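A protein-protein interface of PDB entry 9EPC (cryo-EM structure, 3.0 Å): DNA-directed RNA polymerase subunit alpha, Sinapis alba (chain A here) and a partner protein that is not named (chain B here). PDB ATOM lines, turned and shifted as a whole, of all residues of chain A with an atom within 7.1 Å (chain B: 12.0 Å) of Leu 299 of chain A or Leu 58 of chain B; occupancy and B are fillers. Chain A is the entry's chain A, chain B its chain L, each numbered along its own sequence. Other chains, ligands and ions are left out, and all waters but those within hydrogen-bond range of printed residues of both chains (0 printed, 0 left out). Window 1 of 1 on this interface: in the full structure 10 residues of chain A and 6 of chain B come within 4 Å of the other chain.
The backbone NH of Leu 58 of chain B is in hydrogen-bond range of the backbone carbonyl oxygen of Leu 299 of chain A (3.0 Å). The backbone NH (N) of Leu 58 of chain B lies within hydrogen-bond range of the backbone carbonyl oxygen (O) of Asn 301 of chain A (2.9 Å). The side-chain amide oxygen (OE1) of Gln 303 of chain A sits close to the backbone carbonyl oxygen (O) of Pro 57 of chain B (3.4 Å). The backbone carbonyl oxygen of Gln 60 of chain B lies within hydrogen-bond range of the side-chain amide nitrogen of Gln 303 of chain A, at 2.7 Å. NE2 of Gln 303 of chain A sits close to O of Leu 58 of chain B (2.3 Å).
The backbone NH (N) of Leu 296 of chain A lies within hydrogen-bond range of the backbone carbonyl oxygen (O) of Phe 269 of chain A, at 3.4 Å. The side-chain amide nitrogen (ND2) of Asn 300 of chain A sits close to the backbone carbonyl oxygen (O) of Leu 296 of chain A (3.2 Å). The backbone carbonyl oxygen of Asp 297 of chain A sits close to the side-chain amide oxygen of Asn 301 of chain A (2.9 Å). The backbone carbonyl oxygen (O) of Pro 55 of chain B is in hydrogen-bond range of the side-chain amide nitrogen (NE2) of Gln 60 of chain B (2.5 Å).
Among the printed residues, merely in contact across the chains: Leu 299 of chain A with Pro 57 of chain B, Asn 301 of chain A with Pro 57 of chain B, Gln 303 of chain A with Ser 61 of chain B, Leu 298 of chain A with Leu 58 of chain B, Asn 300 of chain A with Pro 57 of chain B, Gln 303 of chain A with Phe 59 of chain B, Leu 324 of chain A with Leu 58 of chain B, Leu 299 of chain A with Phe 56 of chain B, Leu 321 of chain A with Leu 58 of chain B, Phe 269 of chain A with Phe 56 of chain B and Ser 302 of chain A with Pro 57 of chain B.
Printed residues of chain B within 4 Å of Leu 299 of chain A: Phe 56, Pro 57 and Leu 58. Leu 58 of chain B touches six residues of chain A. Of chain B, only Phe 56 comes within 4 Å of Phe 269 of chain A. No residue of chain B comes within 4 Å of Leu 296 of chain A. Asn 300 of chain A touches just one residue of chain B: Pro 57 (3.6 Å). Printed residues of chain B within 4 Å of Ser 302 of chain A: Pro 57 (3.9 Å). Gln 303 of chain A touches just these residues of chain B: Pro 57 (3.4 Å), Leu 58 (2.3 Å), Phe 59 (3.6 Å), Gln 60 (2.7 Å) and Ser 61 (3.5 Å). Leu 321 of chain A touches just one residue of chain B: Leu 58 (3.8 Å). Of the printed residues of chain A, Phe 56 of chain B touches Phe 269 and Leu 299. Of the printed residues of chain A, Pro 57 of chain B touches Leu 299 (3.3 Å), Asn 300 (3.6 Å), Asn 301 (3.3 Å), Ser 302 (3.9 Å) and Gln 303 (3.4 Å). Leu 320 of chain A touches none of the printed residues of chain B. The nearest residue of chain B that does not touch Leu 299 of chain A is Phe 59 of chain B (4.3 Å). The nearest printed residue of chain A that does not touch Phe 56 of chain B is Leu 296 of chain A (4.3 Å).
Hydrophobic or aromatic side chains of chain B that line the printed part of chain A: Phe 56, Pro 57 and Leu 58. Along chain B the printed residues that touch a printed residue of chain A span positions 56 to 61. Hydrophobic or aromatic side chains of chain A that line the printed part of chain B: Phe 269, Leu 298, Leu 299, Leu 321 and Leu 324. Among the printed residues, 16 pairs touch across the chains.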
ATOM      1  N   PHE A 269      11.799 -22.327  -7.900  1.00  0.00           N
ATOM      2  CA  PHE A 269      12.162 -23.138  -6.743  1.00  0.00           C
ATOM      3  C   PHE A 269      10.964 -23.872  -6.161  1.00  0.00           C
ATOM      4  O   PHE A 269      11.132 -24.915  -5.521  1.00  0.00           O
ATOM      5  CB  PHE A 269      12.818 -22.265  -5.675  1.00  0.00           C
ATOM      6  CG  PHE A 269      14.223 -21.865  -6.004  1.00  0.00           C
ATOM      7  CD1 PHE A 269      14.939 -22.539  -6.979  1.00  0.00           C
ATOM      8  CD2 PHE A 269      14.836 -20.821  -5.334  1.00  0.00           C
ATOM      9  CE1 PHE A 269      16.234 -22.177  -7.282  1.00  0.00           C
ATOM     10  CE2 PHE A 269      16.132 -20.455  -5.632  1.00  0.00           C
ATOM     11  CZ  PHE A 269      16.831 -21.133  -6.607  1.00  0.00           C
ATOM     12  N   ILE A 292       8.631 -31.012   4.818  1.00  0.00           N
ATOM     13  CA  ILE A 292       9.405 -30.143   3.941  1.00  0.00           C
ATOM     14  C   ILE A 292       9.690 -30.946   2.680  1.00  0.00           C
ATOM     15  O   ILE A 292      10.536 -31.846   2.681  1.00  0.00           O
ATOM     16  CB  ILE A 292      10.699 -29.662   4.602  1.00  0.00           C
ATOM     17  CG1 ILE A 292      10.406 -29.083   5.985  1.00  0.00           C
ATOM     18  CG2 ILE A 292      11.386 -28.631   3.727  1.00  0.00           C
ATOM     19  CD1 ILE A 292      11.647 -28.772   6.783  1.00  0.00           C
ATOM     20  N   THR A 294       9.550 -29.317  -0.845  1.00  0.00           N
ATOM     21  CA  THR A 294      10.061 -28.505  -1.936  1.00  0.00           C
ATOM     22  C   THR A 294      11.330 -27.779  -1.509  1.00  0.00           C
ATOM     23  O   THR A 294      11.560 -27.523  -0.325  1.00  0.00           O
ATOM     24  CB  THR A 294       9.006 -27.492  -2.387  1.00  0.00           C
ATOM     25  OG1 THR A 294       7.711 -28.100  -2.335  1.00  0.00           O
ATOM     26  CG2 THR A 294       9.274 -27.042  -3.804  1.00  0.00           C
ATOM     27  N   LEU A 295      12.164 -27.455  -2.498  1.00  0.00           N
ATOM     28  CA  LEU A 295      13.357 -26.664  -2.223  1.00  0.00           C
ATOM     29  C   LEU A 295      12.988 -25.283  -1.699  1.00  0.00           C
ATOM     30  O   LEU A 295      13.649 -24.757  -0.798  1.00  0.00           O
ATOM     31  CB  LEU A 295      14.218 -26.559  -3.482  1.00  0.00           C
ATOM     32  CG  LEU A 295      15.529 -25.778  -3.402  1.00  0.00           C
ATOM     33  CD1 LEU A 295      16.599 -26.474  -4.215  1.00  0.00           C
ATOM     34  CD2 LEU A 295      15.334 -24.364  -3.907  1.00  0.00           C
ATOM     35  N   LEU A 296      11.933 -24.682  -2.254  1.00  0.00           N
ATOM     36  CA  LEU A 296      11.486 -23.381  -1.768  1.00  0.00           C
ATOM     37  C   LEU A 296      11.063 -23.454  -0.307  1.00  0.00           C
ATOM     38  O   LEU A 296      11.379 -22.557   0.484  1.00  0.00           O
ATOM     39  CB  LEU A 296      10.335 -22.864  -2.628  1.00  0.00           C
ATOM     40  CG  LEU A 296       9.757 -21.522  -2.182  1.00  0.00           C
ATOM     41  CD1 LEU A 296      10.818 -20.439  -2.255  1.00  0.00           C
ATOM     42  CD2 LEU A 296       8.546 -21.148  -3.017  1.00  0.00           C
ATOM     43  N   ASP A 297      10.341 -24.510   0.070  1.00  0.00           N
ATOM     44  CA  ASP A 297       9.981 -24.693   1.471  1.00  0.00           C
ATOM     45  C   ASP A 297      11.216 -24.883   2.340  1.00  0.00           C
ATOM     46  O   ASP A 297      11.250 -24.410   3.482  1.00  0.00           O
ATOM     47  CB  ASP A 297       9.035 -25.883   1.624  1.00  0.00           C
ATOM     48  CG  ASP A 297       7.685 -25.639   0.980  1.00  0.00           C
ATOM     49  OD1 ASP A 297       7.626 -25.522  -0.261  1.00  0.00           O
ATOM     50  OD2 ASP A 297       6.679 -25.565   1.716  1.00  0.00           O
ATOM     51  N   LEU A 298      12.231 -25.577   1.825  1.00  0.00           N
ATOM     52  CA  LEU A 298      13.473 -25.736   2.573  1.00  0.00           C
ATOM     53  C   LEU A 298      14.168 -24.397   2.781  1.00  0.00           C
ATOM     54  O   LEU A 298      14.694 -24.128   3.867  1.00  0.00           O
ATOM     55  CB  LEU A 298      14.399 -26.711   1.850  1.00  0.00           C
ATOM     56  CG  LEU A 298      15.764 -26.931   2.499  1.00  0.00           C
ATOM     57  CD1 LEU A 298      15.603 -27.488   3.901  1.00  0.00           C
ATOM     58  CD2 LEU A 298      16.616 -27.853   1.647  1.00  0.00           C
ATOM     59  N   LEU A 299      14.183 -23.547   1.753  1.00  0.00           N
ATOM     60  CA  LEU A 299      14.852 -22.256   1.875  1.00  0.00           C
ATOM     61  C   LEU A 299      14.142 -21.341   2.863  1.00  0.00           C
ATOM     62  O   LEU A 299      14.800 -20.579   3.579  1.00  0.00           O
ATOM     63  CB  LEU A 299      14.951 -21.583   0.508  1.00  0.00           C
ATOM     64  CG  LEU A 299      15.794 -22.315  -0.537  1.00  0.00           C
ATOM     65  CD1 LEU A 299      15.970 -21.454  -1.775  1.00  0.00           C
ATOM     66  CD2 LEU A 299      17.140 -22.716   0.041  1.00  0.00           C
ATOM     67  N   ASN A 300      12.811 -21.398   2.919  1.00  0.00           N
ATOM     68  CA  ASN A 300      12.065 -20.536   3.828  1.00  0.00           C
ATOM     69  C   ASN A 300      12.323 -20.853   5.293  1.00  0.00           C
ATOM     70  O   ASN A 300      12.007 -20.024   6.151  1.00  0.00           O
ATOM     71  CB  ASN A 300      10.568 -20.635   3.536  1.00  0.00           C
ATOM     72  CG  ASN A 300      10.209 -20.105   2.165  1.00  0.00           C
ATOM     73  OD1 ASN A 300      10.909 -19.257   1.612  1.00  0.00           O
ATOM     74  ND2 ASN A 300       9.112 -20.601   1.608  1.00  0.00           N
ATOM     75  N   ASN A 301      12.879 -22.020   5.602  1.00  0.00           N
ATOM     76  CA  ASN A 301      13.230 -22.340   6.973  1.00  0.00           C
ATOM     77  C   ASN A 301      14.586 -21.738   7.332  1.00  0.00           C
ATOM     78  O   ASN A 301      15.351 -21.298   6.470  1.00  0.00           O
ATOM     79  CB  ASN A 301      13.246 -23.851   7.185  1.00  0.00           C
ATOM     80  CG  ASN A 301      11.873 -24.469   7.056  1.00  0.00           C
ATOM     81  OD1 ASN A 301      11.013 -23.956   6.343  1.00  0.00           O
ATOM     82  ND2 ASN A 301      11.657 -25.576   7.753  1.00  0.00           N
ATOM     83  N   SER A 302      14.879 -21.720   8.627  1.00  0.00           N
ATOM     84  CA  SER A 302      16.139 -21.213   9.145  1.00  0.00           C
ATOM     85  C   SER A 302      16.951 -22.350   9.750  1.00  0.00           C
ATOM     86  O   SER A 302      16.441 -23.448   9.988  1.00  0.00           O
ATOM     87  CB  SER A 302      15.904 -20.123  10.195  1.00  0.00           C
ATOM     88  OG  SER A 302      15.213 -20.642  11.316  1.00  0.00           O
ATOM     89  N   GLN A 303      18.232 -22.069   9.997  1.00  0.00           N
ATOM     90  CA  GLN A 303      19.104 -23.075  10.594  1.00  0.00           C
ATOM     91  C   GLN A 303      18.602 -23.484  11.971  1.00  0.00           C
ATOM     92  O   GLN A 303      18.595 -24.673  12.310  1.00  0.00           O
ATOM     93  CB  GLN A 303      20.538 -22.553  10.679  1.00  0.00           C
ATOM     94  CG  GLN A 303      21.184 -22.242   9.338  1.00  0.00           C
ATOM     95  CD  GLN A 303      20.762 -20.898   8.778  1.00  0.00           C
ATOM     96  OE1 GLN A 303      19.757 -20.322   9.197  1.00  0.00           O
ATOM     97  NE2 GLN A 303      21.534 -20.387   7.826  1.00  0.00           N
ATOM     98  N   GLU A 304      18.174 -22.511  12.778  1.00  0.00           N
ATOM     99  CA  GLU A 304      17.577 -22.835  14.069  1.00  0.00           C
ATOM    100  C   GLU A 304      16.305 -23.652  13.891  1.00  0.00           C
ATOM    101  O   GLU A 304      16.041 -24.582  14.662  1.00  0.00           O
ATOM    102  CB  GLU A 304      17.293 -21.552  14.852  1.00  0.00           C
ATOM    103  CG  GLU A 304      16.463 -21.759  16.109  1.00  0.00           C
ATOM    104  CD  GLU A 304      17.118 -22.704  17.097  1.00  0.00           C
ATOM    105  OE1 GLU A 304      18.365 -22.725  17.171  1.00  0.00           O
ATOM    106  OE2 GLU A 304      16.384 -23.431  17.800  1.00  0.00           O
ATOM    107  N   LEU A 306      15.854 -25.785  11.728  1.00  0.00           N
ATOM    108  CA  LEU A 306      16.261 -27.138  11.375  1.00  0.00           C
ATOM    109  C   LEU A 306      16.898 -27.882  12.539  1.00  0.00           C
ATOM    110  O   LEU A 306      16.745 -29.105  12.639  1.00  0.00           O
ATOM    111  CB  LEU A 306      17.240 -27.109  10.199  1.00  0.00           C
ATOM    112  CG  LEU A 306      16.657 -27.313   8.799  1.00  0.00           C
ATOM    113  CD1 LEU A 306      15.585 -26.283   8.496  1.00  0.00           C
ATOM    114  CD2 LEU A 306      17.759 -27.258   7.759  1.00  0.00           C
ATOM    115  N   VAL A 317      23.444 -29.230   9.221  1.00  0.00           N
ATOM    116  CA  VAL A 317      23.058 -28.005   8.529  1.00  0.00           C
ATOM    117  C   VAL A 317      24.235 -27.443   7.745  1.00  0.00           C
ATOM    118  O   VAL A 317      24.047 -26.755   6.734  1.00  0.00           O
ATOM    119  CB  VAL A 317      22.484 -26.973   9.522  1.00  0.00           C
ATOM    120  CG1 VAL A 317      23.584 -26.359  10.369  1.00  0.00           C
ATOM    121  CG2 VAL A 317      21.713 -25.894   8.779  1.00  0.00           C
ATOM    122  N   LEU A 320      24.421 -29.633   4.614  1.00  0.00           N
ATOM    123  CA  LEU A 320      23.248 -29.362   3.791  1.00  0.00           C
ATOM    124  C   LEU A 320      23.436 -28.098   2.962  1.00  0.00           C
ATOM    125  O   LEU A 320      23.014 -28.043   1.800  1.00  0.00           O
ATOM    126  CB  LEU A 320      22.006 -29.249   4.673  1.00  0.00           C
ATOM    127  CG  LEU A 320      20.696 -28.912   3.960  1.00  0.00           C
ATOM    128  CD1 LEU A 320      20.400 -29.937   2.882  1.00  0.00           C
ATOM    129  CD2 LEU A 320      19.555 -28.839   4.955  1.00  0.00           C
ATOM    130  N   LEU A 321      24.064 -27.073   3.541  1.00  0.00           N
ATOM    131  CA  LEU A 321      24.213 -25.802   2.840  1.00  0.00           C
ATOM    132  C   LEU A 321      25.091 -25.947   1.604  1.00  0.00           C
ATOM    133  O   LEU A 321      24.723 -25.498   0.514  1.00  0.00           O
ATOM    134  CB  LEU A 321      24.783 -24.747   3.787  1.00  0.00           C
ATOM    135  CG  LEU A 321      23.799 -24.171   4.804  1.00  0.00           C
ATOM    136  CD1 LEU A 321      24.499 -23.213   5.749  1.00  0.00           C
ATOM    137  CD2 LEU A 321      22.648 -23.478   4.093  1.00  0.00           C
ATOM    138  N   LEU A 324      23.454 -27.309  -1.383  1.00  0.00           N
ATOM    139  CA  LEU A 324      22.702 -26.273  -2.079  1.00  0.00           C
ATOM    140  C   LEU A 324      23.623 -25.301  -2.802  1.00  0.00           C
ATOM    141  O   LEU A 324      23.256 -24.772  -3.857  1.00  0.00           O
ATOM    142  CB  LEU A 324      21.812 -25.524  -1.091  1.00  0.00           C
ATOM    143  CG  LEU A 324      20.775 -26.375  -0.359  1.00  0.00           C
ATOM    144  CD1 LEU A 324      20.189 -25.608   0.807  1.00  0.00           C
ATOM    145  CD2 LEU A 324      19.679 -26.805  -1.317  1.00  0.00           C
ATOM    146  N   PRO B  55      19.635 -14.617  -0.161  1.00  0.00           N
ATOM    147  CA  PRO B  55      18.921 -13.850   0.866  1.00  0.00           C
ATOM    148  C   PRO B  55      17.834 -14.670   1.552  1.00  0.00           C
ATOM    149  O   PRO B  55      17.077 -14.134   2.361  1.00  0.00           O
ATOM    150  CB  PRO B  55      18.311 -12.696   0.072  1.00  0.00           C
ATOM    151  CG  PRO B  55      18.098 -13.266  -1.286  1.00  0.00           C
ATOM    152  CD  PRO B  55      19.253 -14.201  -1.522  1.00  0.00           C
ATOM    153  N   PHE B  56      17.764 -15.956   1.223  1.00  0.00           N
ATOM    154  CA  PHE B  56      16.767 -16.822   1.824  1.00  0.00           C
ATOM    155  C   PHE B  56      17.075 -17.041   3.306  1.00  0.00           C
ATOM    156  O   PHE B  56      18.232 -16.959   3.725  1.00  0.00           O
ATOM    157  CB  PHE B  56      16.716 -18.162   1.099  1.00  0.00           C
ATOM    158  CG  PHE B  56      16.191 -18.069  -0.304  1.00  0.00           C
ATOM    159  CD1 PHE B  56      14.829 -18.041  -0.544  1.00  0.00           C
ATOM    160  CD2 PHE B  56      17.058 -18.010  -1.379  1.00  0.00           C
ATOM    161  CE1 PHE B  56      14.341 -17.954  -1.831  1.00  0.00           C
ATOM    162  CE2 PHE B  56      16.576 -17.923  -2.670  1.00  0.00           C
ATOM    163  CZ  PHE B  56      15.215 -17.896  -2.895  1.00  0.00           C
ATOM    164  N   PRO B  57      16.051 -17.312   4.119  1.00  0.00           N
ATOM    165  CA  PRO B  57      16.296 -17.528   5.553  1.00  0.00           C
ATOM    166  C   PRO B  57      17.260 -18.663   5.841  1.00  0.00           C
ATOM    167  O   PRO B  57      17.972 -18.616   6.850  1.00  0.00           O
ATOM    168  CB  PRO B  57      14.895 -17.825   6.103  1.00  0.00           C
ATOM    169  CG  PRO B  57      13.972 -17.153   5.150  1.00  0.00           C
ATOM    170  CD  PRO B  57      14.613 -17.291   3.801  1.00  0.00           C
ATOM    171  N   LEU B  58      17.300 -19.690   4.991  1.00  0.00           N
ATOM    172  CA  LEU B  58      18.235 -20.786   5.214  1.00  0.00           C
ATOM    173  C   LEU B  58      19.676 -20.336   5.006  1.00  0.00           C
ATOM    174  O   LEU B  58      20.573 -20.748   5.750  1.00  0.00           O
ATOM    175  CB  LEU B  58      17.898 -21.959   4.297  1.00  0.00           C
ATOM    176  CG  LEU B  58      18.699 -23.235   4.549  1.00  0.00           C
ATOM    177  CD1 LEU B  58      18.546 -23.677   5.992  1.00  0.00           C
ATOM    178  CD2 LEU B  58      18.253 -24.332   3.603  1.00  0.00           C
ATOM    179  N   PHE B  59      19.921 -19.498   3.997  1.00  0.00           N
ATOM    180  CA  PHE B  59      21.279 -19.020   3.757  1.00  0.00           C
ATOM    181  C   PHE B  59      21.727 -18.056   4.848  1.00  0.00           C
ATOM    182  O   PHE B  59      22.866 -18.134   5.322  1.00  0.00           O
ATOM    183  CB  PHE B  59      21.367 -18.362   2.382  1.00  0.00           C
ATOM    184  CG  PHE B  59      21.263 -19.333   1.244  1.00  0.00           C
ATOM    185  CD1 PHE B  59      21.629 -20.657   1.412  1.00  0.00           C
ATOM    186  CD2 PHE B  59      20.798 -18.923   0.006  1.00  0.00           C
ATOM    187  CE1 PHE B  59      21.536 -21.555   0.369  1.00  0.00           C
ATOM    188  CE2 PHE B  59      20.701 -19.817  -1.043  1.00  0.00           C
ATOM    189  CZ  PHE B  59      21.070 -21.135  -0.861  1.00  0.00           C
ATOM    190  N   GLN B  60      20.852 -17.137   5.252  1.00  0.00           N
ATOM    191  CA  GLN B  60      21.159 -16.251   6.366  1.00  0.00           C
ATOM    192  C   GLN B  60      21.327 -17.066   7.642  1.00  0.00           C
ATOM    193  O   GLN B  60      20.509 -17.939   7.943  1.00  0.00           O
ATOM    194  CB  GLN B  60      20.050 -15.218   6.536  1.00  0.00           C
ATOM    195  CG  GLN B  60      19.746 -14.429   5.276  1.00  0.00           C
ATOM    196  CD  GLN B  60      18.457 -13.640   5.382  1.00  0.00           C
ATOM    197  OE1 GLN B  60      17.776 -13.678   6.408  1.00  0.00           O
ATOM    198  NE2 GLN B  60      18.111 -12.925   4.319  1.00  0.00           N
ATOM    199  N   SER B  61      22.385 -16.779   8.395  1.00  0.00           N
ATOM    200  CA  SER B  61      22.747 -17.563   9.576  1.00  0.00           C
ATOM    201  C   SER B  61      22.939 -16.649  10.779  1.00  0.00           C
ATOM    202  O   SER B  61      24.069 -16.410  11.220  1.00  0.00           O
ATOM    203  CB  SER B  61      24.010 -18.385   9.313  1.00  0.00           C
ATOM    204  OG  SER B  61      25.111 -17.543   9.022  1.00  0.00           O
ATOM    205  N   PRO B  62      21.848 -16.117  11.338  1.00  0.00           N
ATOM    206  CA  PRO B  62      21.968 -15.386  12.608  1.00  0.00           C
ATOM    207  C   PRO B  62      22.407 -16.265  13.764  1.00  0.00           C
ATOM    208  O   PRO B  62      22.929 -15.742  14.756  1.00  0.00           O
ATOM    209  CB  PRO B  62      20.553 -14.833  12.837  1.00  0.00           C
ATOM    210  CG  PRO B  62      19.883 -14.905  11.499  1.00  0.00           C
ATOM    211  CD  PRO B  62      20.466 -16.109  10.833  1.00  0.00           C
ATOM    212  N   ALA B  63      22.215 -17.577  13.667  1.00  0.00           N
ATOM    213  CA  ALA B  63      22.599 -18.495  14.732  1.00  0.00           C
ATOM    214  C   ALA B  63      23.235 -19.753  14.153  1.00  0.00           C
ATOM    215  O   ALA B  63      23.225 -19.965  12.940  1.00  0.00           O
ATOM    216  CB  ALA B  63      21.393 -18.851  15.585  1.00  0.00           C
